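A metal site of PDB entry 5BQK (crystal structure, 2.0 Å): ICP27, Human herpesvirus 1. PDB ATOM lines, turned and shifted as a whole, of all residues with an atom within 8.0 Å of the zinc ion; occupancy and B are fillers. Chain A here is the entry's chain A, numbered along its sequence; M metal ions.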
ATOM      1  N   PRO A 155      28.632  29.847 -28.732  1.00  0.00           N
ATOM      2  CA  PRO A 155      28.657  29.795 -27.258  1.00  0.00           C
ATOM      3  C   PRO A 155      29.032  28.402 -26.672  1.00  0.00           C
ATOM      4  O   PRO A 155      29.600  28.286 -25.540  1.00  0.00           O
ATOM      5  CB  PRO A 155      27.220  30.186 -26.860  1.00  0.00           C
ATOM      6  CG  PRO A 155      26.394  29.759 -28.088  1.00  0.00           C
ATOM      7  CD  PRO A 155      27.297  30.135 -29.267  1.00  0.00           C
ATOM      8  N   PHE A 156      28.724  27.372 -27.441  1.00  0.00           N
ATOM      9  CA  PHE A 156      29.137  26.012 -27.112  1.00  0.00           C
ATOM     10  C   PHE A 156      30.640  25.830 -27.252  1.00  0.00           C
ATOM     11  O   PHE A 156      31.279  25.255 -26.355  1.00  0.00           O
ATOM     12  CB  PHE A 156      28.376  24.987 -27.982  1.00  0.00           C
ATOM     13  CG  PHE A 156      28.976  23.573 -27.912  1.00  0.00           C
ATOM     14  CD1 PHE A 156      28.616  22.705 -26.887  1.00  0.00           C
ATOM     15  CD2 PHE A 156      29.942  23.157 -28.844  1.00  0.00           C
ATOM     16  CE1 PHE A 156      29.170  21.409 -26.790  1.00  0.00           C
ATOM     17  CE2 PHE A 156      30.540  21.854 -28.770  1.00  0.00           C
ATOM     18  CZ  PHE A 156      30.167  20.987 -27.741  1.00  0.00           C
ATOM     19  N   LEU A 157      31.207  26.302 -28.382  1.00  0.00           N
ATOM     20  CA  LEU A 157      32.652  26.254 -28.582  1.00  0.00           C
ATOM     21  C   LEU A 157      33.406  27.093 -27.546  1.00  0.00           C
ATOM     22  O   LEU A 157      34.505  26.670 -27.134  1.00  0.00           O
ATOM     23  CB  LEU A 157      33.072  26.598 -30.003  1.00  0.00           C
ATOM     24  CG  LEU A 157      32.581  25.623 -31.076  1.00  0.00           C
ATOM     25  CD1 LEU A 157      32.775  26.199 -32.491  1.00  0.00           C
ATOM     26  CD2 LEU A 157      33.256  24.221 -30.957  1.00  0.00           C
ATOM     27  N   GLN A 158      32.832  28.183 -27.043  1.00  0.00           N
ATOM     28  CA  GLN A 158      33.547  28.931 -26.033  1.00  0.00           C
ATOM     29  C   GLN A 158      33.948  27.925 -24.894  1.00  0.00           C
ATOM     30  O   GLN A 158      35.092  27.902 -24.437  1.00  0.00           O
ATOM     31  CB  GLN A 158      32.768  30.108 -25.479  1.00  0.00           C
ATOM     32  CG  GLN A 158      33.725  31.096 -24.631  1.00  0.00           C
ATOM     33  N   CYS A 159      33.007  27.046 -24.518  1.00  0.00           N
ATOM     34  CA  CYS A 159      33.231  26.110 -23.420  1.00  0.00           C
ATOM     35  C   CYS A 159      34.090  24.910 -23.859  1.00  0.00           C
ATOM     36  O   CYS A 159      35.094  24.579 -23.230  1.00  0.00           O
ATOM     37  CB  CYS A 159      31.897  25.712 -22.755  1.00  0.00           C
ATOM     38  SG  CYS A 159      31.990  24.579 -21.207  1.00  0.00           S
ATOM     39  N   TYR A 160      33.684  24.254 -24.930  1.00  0.00           N
ATOM     40  CA  TYR A 160      34.329  23.088 -25.420  1.00  0.00           C
ATOM     41  C   TYR A 160      35.822  23.311 -25.753  1.00  0.00           C
ATOM     42  O   TYR A 160      36.685  22.454 -25.432  1.00  0.00           O
ATOM     43  CB  TYR A 160      33.582  22.619 -26.695  1.00  0.00           C
ATOM     44  CG  TYR A 160      34.337  21.566 -27.442  1.00  0.00           C
ATOM     45  CD1 TYR A 160      34.264  20.214 -27.061  1.00  0.00           C
ATOM     46  CD2 TYR A 160      35.123  21.903 -28.514  1.00  0.00           C
ATOM     47  CE1 TYR A 160      34.948  19.200 -27.783  1.00  0.00           C
ATOM     48  CE2 TYR A 160      35.840  20.930 -29.218  1.00  0.00           C
ATOM     49  CZ  TYR A 160      35.745  19.573 -28.833  1.00  0.00           C
ATOM     50  OH  TYR A 160      36.433  18.593 -29.549  1.00  0.00           O
ATOM     51  N   LEU A 161      36.129  24.432 -26.391  1.00  0.00           N
ATOM     52  CA  LEU A 161      37.514  24.668 -26.902  1.00  0.00           C
ATOM     53  C   LEU A 161      38.400  24.932 -25.662  1.00  0.00           C
ATOM     54  O   LEU A 161      39.548  24.468 -25.597  1.00  0.00           O
ATOM     55  CB  LEU A 161      37.583  25.834 -27.882  1.00  0.00           C
ATOM     56  CG  LEU A 161      36.966  25.608 -29.290  1.00  0.00           C
ATOM     57  CD1 LEU A 161      37.074  26.899 -30.065  1.00  0.00           C
ATOM     58  CD2 LEU A 161      37.709  24.492 -30.041  1.00  0.00           C
ATOM     59  N   ALA A 163      37.865  23.480 -22.803  1.00  0.00           N
ATOM     60  CA  ALA A 163      38.034  22.109 -22.270  1.00  0.00           C
ATOM     61  C   ALA A 163      39.069  21.337 -23.024  1.00  0.00           C
ATOM     62  O   ALA A 163      39.752  20.537 -22.430  1.00  0.00           O
ATOM     63  CB  ALA A 163      36.683  21.323 -22.193  1.00  0.00           C
ATOM     64  N   HIS A 238      30.453  16.156 -24.953  1.00  0.00           N
ATOM     65  CA  HIS A 238      31.073  17.171 -24.102  1.00  0.00           C
ATOM     66  C   HIS A 238      30.394  17.295 -22.723  1.00  0.00           C
ATOM     67  O   HIS A 238      31.040  17.664 -21.694  1.00  0.00           O
ATOM     68  CB  HIS A 238      31.186  18.526 -24.839  1.00  0.00           C
ATOM     69  CG  HIS A 238      31.523  19.691 -23.945  1.00  0.00           C
ATOM     70  ND1 HIS A 238      32.803  19.935 -23.487  1.00  0.00           N
ATOM     71  CD2 HIS A 238      30.737  20.628 -23.363  1.00  0.00           C
ATOM     72  CE1 HIS A 238      32.804  21.035 -22.741  1.00  0.00           C
ATOM     73  NE2 HIS A 238      31.553  21.479 -22.649  1.00  0.00           N
ATOM     74  N   ARG A 239      29.094  17.038 -22.673  1.00  0.00           N
ATOM     75  CA  ARG A 239      28.361  17.169 -21.437  1.00  0.00           C
ATOM     76  C   ARG A 239      28.880  16.145 -20.379  1.00  0.00           C
ATOM     77  O   ARG A 239      28.645  16.332 -19.191  1.00  0.00           O
ATOM     78  CB  ARG A 239      26.833  17.012 -21.640  1.00  0.00           C
ATOM     79  CG  ARG A 239      26.432  15.589 -21.976  1.00  0.00           C
ATOM     80  CD  ARG A 239      25.078  15.434 -22.633  1.00  0.00           C
ATOM     81  NE  ARG A 239      24.998  16.002 -23.984  1.00  0.00           N
ATOM     82  CZ  ARG A 239      23.899  16.525 -24.532  1.00  0.00           C
ATOM     83  NH1 ARG A 239      22.762  16.618 -23.838  1.00  0.00           N
ATOM     84  NH2 ARG A 239      23.935  16.986 -25.784  1.00  0.00           N
ATOM     85  N   GLN A 240      29.575  15.092 -20.839  1.00  0.00           N
ATOM     86  CA  GLN A 240      30.164  14.087 -19.941  1.00  0.00           C
ATOM     87  C   GLN A 240      31.353  14.655 -19.207  1.00  0.00           C
ATOM     88  O   GLN A 240      31.613  14.221 -18.114  1.00  0.00           O
ATOM     89  CB  GLN A 240      30.569  12.829 -20.695  1.00  0.00           C
ATOM     90  CG  GLN A 240      29.376  11.953 -21.029  1.00  0.00           C
ATOM     91  CD  GLN A 240      29.588  11.007 -22.243  1.00  0.00           C
ATOM     92  OE1 GLN A 240      28.710  10.193 -22.534  1.00  0.00           O
ATOM     93  NE2 GLN A 240      30.707  11.131 -22.950  1.00  0.00           N
ATOM     94  N   GLU A 241      32.075  15.612 -19.831  1.00  0.00           N
ATOM     95  CA  GLU A 241      33.220  16.260 -19.191  1.00  0.00           C
ATOM     96  C   GLU A 241      32.917  17.641 -18.572  1.00  0.00           C
ATOM     97  O   GLU A 241      33.825  18.322 -18.038  1.00  0.00           O
ATOM     98  CB  GLU A 241      34.452  16.351 -20.134  1.00  0.00           C
ATOM     99  CG  GLU A 241      34.403  17.537 -21.155  1.00  0.00           C
ATOM    100  CD  GLU A 241      35.409  17.393 -22.293  1.00  0.00           C
ATOM    101  OE1 GLU A 241      36.612  17.392 -22.005  1.00  0.00           O
ATOM    102  OE2 GLU A 241      35.000  17.318 -23.484  1.00  0.00           O
ATOM    103  N   CYS A 242      31.663  18.078 -18.612  1.00  0.00           N
ATOM    104  CA  CYS A 242      31.412  19.475 -18.337  1.00  0.00           C
ATOM    105  C   CYS A 242      30.278  19.530 -17.345  1.00  0.00           C
ATOM    106  O   CYS A 242      29.224  18.924 -17.598  1.00  0.00           O
ATOM    107  CB  CYS A 242      31.040  20.198 -19.667  1.00  0.00           C
ATOM    108  SG  CYS A 242      30.473  21.883 -19.476  1.00  0.00           S
ATOM    109  N   SER A 243      30.486  20.235 -16.221  1.00  0.00           N
ATOM    110  CA  SER A 243      29.435  20.315 -15.200  1.00  0.00           C
ATOM    111  C   SER A 243      28.434  21.515 -15.393  1.00  0.00           C
ATOM    112  O   SER A 243      27.593  21.762 -14.527  1.00  0.00           O
ATOM    113  CB  SER A 243      30.035  20.370 -13.778  1.00  0.00           C
ATOM    114  OG  SER A 243      30.883  21.498 -13.681  1.00  0.00           O
ATOM    115  N   SER A 244      28.530  22.253 -16.479  1.00  0.00           N
ATOM    116  CA  SER A 244      27.602  23.374 -16.710  1.00  0.00           C
ATOM    117  C   SER A 244      26.254  22.943 -17.307  1.00  0.00           C
ATOM    118  O   SER A 244      26.200  22.441 -18.415  1.00  0.00           O
ATOM    119  CB  SER A 244      28.283  24.443 -17.582  1.00  0.00           C
ATOM    120  OG  SER A 244      27.317  25.303 -18.125  1.00  0.00           O
ATOM    121  N   ARG A 245      25.174  23.193 -16.567  1.00  0.00           N
ATOM    122  CA  ARG A 245      23.784  23.041 -17.004  1.00  0.00           C
ATOM    123  C   ARG A 245      23.484  23.954 -18.223  1.00  0.00           C
ATOM    124  O   ARG A 245      22.811  23.515 -19.165  1.00  0.00           O
ATOM    125  CB  ARG A 245      22.781  23.345 -15.841  1.00  0.00           C
ATOM    126  CG  ARG A 245      21.232  23.325 -16.177  1.00  0.00           C
ATOM    127  CD  ARG A 245      20.762  21.939 -16.820  1.00  0.00           C
ATOM    128  NE  ARG A 245      19.310  21.889 -17.055  1.00  0.00           N
ATOM    129  CZ  ARG A 245      18.644  20.866 -17.617  1.00  0.00           C
ATOM    130  NH1 ARG A 245      19.261  19.756 -18.002  1.00  0.00           N
ATOM    131  NH2 ARG A 245      17.319  20.926 -17.746  1.00  0.00           N
ATOM    132  N   VAL A 246      23.963  25.204 -18.206  1.00  0.00           N
ATOM    133  CA  VAL A 246      23.751  26.105 -19.380  1.00  0.00           C
ATOM    134  C   VAL A 246      24.416  25.535 -20.621  1.00  0.00           C
ATOM    135  O   VAL A 246      23.796  25.555 -21.702  1.00  0.00           O
ATOM    136  CB  VAL A 246      24.286  27.517 -19.107  1.00  0.00           C
ATOM    137  CG1 VAL A 246      24.463  28.359 -20.448  1.00  0.00           C
ATOM    138  CG2 VAL A 246      23.414  28.193 -18.072  1.00  0.00           C
ATOM    139  N   CYS A 247      25.638  24.958 -20.462  1.00  0.00           N
ATOM    140  CA  CYS A 247      26.352  24.416 -21.627  1.00  0.00           C
ATOM    141  C   CYS A 247      25.522  23.249 -22.197  1.00  0.00           C
ATOM    142  O   CYS A 247      25.369  23.098 -23.431  1.00  0.00           O
ATOM    143  CB  CYS A 247      27.764  23.892 -21.248  1.00  0.00           C
ATOM    144  SG  CYS A 247      28.663  23.470 -22.659  1.00  0.00           S
ATOM    145  N   GLU A 248      25.033  22.408 -21.279  1.00  0.00           N
ATOM    146  CA  GLU A 248      24.255  21.210 -21.638  1.00  0.00           C
ATOM    147  C   GLU A 248      22.978  21.659 -22.357  1.00  0.00           C
ATOM    148  O   GLU A 248      22.514  21.053 -23.334  1.00  0.00           O
ATOM    149  CB  GLU A 248      23.853  20.429 -20.361  1.00  0.00           C
ATOM    150  CG  GLU A 248      23.179  19.166 -20.722  1.00  0.00           C
ATOM    151  CD  GLU A 248      22.718  18.295 -19.539  1.00  0.00           C
ATOM    152  OE1 GLU A 248      22.583  18.764 -18.381  1.00  0.00           O
ATOM    153  OE2 GLU A 248      22.449  17.111 -19.843  1.00  0.00           O
ATOM    154  N   THR A 250      22.584  24.460 -24.006  1.00  0.00           N
ATOM    155  CA  THR A 250      23.096  24.963 -25.283  1.00  0.00           C
ATOM    156  C   THR A 250      23.350  23.852 -26.279  1.00  0.00           C
ATOM    157  O   THR A 250      22.847  23.866 -27.410  1.00  0.00           O
ATOM    158  CB  THR A 250      24.315  25.863 -25.071  1.00  0.00           C
ATOM    159  OG1 THR A 250      23.923  26.897 -24.156  1.00  0.00           O
ATOM    160  CG2 THR A 250      24.793  26.482 -26.421  1.00  0.00           C
ATOM    161  N   ALA A 251      24.069  22.836 -25.864  1.00  0.00           N
ATOM    162  CA  ALA A 251      24.365  21.766 -26.783  1.00  0.00           C
ATOM    163  C   ALA A 251      23.081  21.045 -27.235  1.00  0.00           C
ATOM    164  O   ALA A 251      22.959  20.641 -28.424  1.00  0.00           O
ATOM    165  CB  ALA A 251      25.308  20.756 -26.136  1.00  0.00           C
HETATM  166 ZN    ZN M   1      30.711  22.928 -21.607  1.00  0.00          ZN
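The backbone NH (N) of Cys 247 sits at hydrogen-bond distance from the side-chain hydroxyl (OG) of Ser 244, 2.9 Å away. The side-chain sulfur of Cys 242 lies close to the backbone NH of Ser 244, at 3.6 Å. A ring nitrogen (ND1) of His 238 is in hydrogen-bond range of the side-chain carboxylate (OE2) of Glu 241, at 3.4 Å.
Within 4 Å of the zinc ion: Cys 159, His 238, Cys 242 and Cys 247. The nearest printed residue that does not touch the zinc ion is Tyr 160 (4.7 Å).
The zinc ion is bound by NE2 of His 238 (2.0 Å). The zinc ion is bound by SG of Cys 159, at 2.1 Å. The zinc ion is bound by the side-chain sulfur (SG) of Cys 247, at 2.4 Å. SG of Cys 242 binds the zinc ion (2.4 Å).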
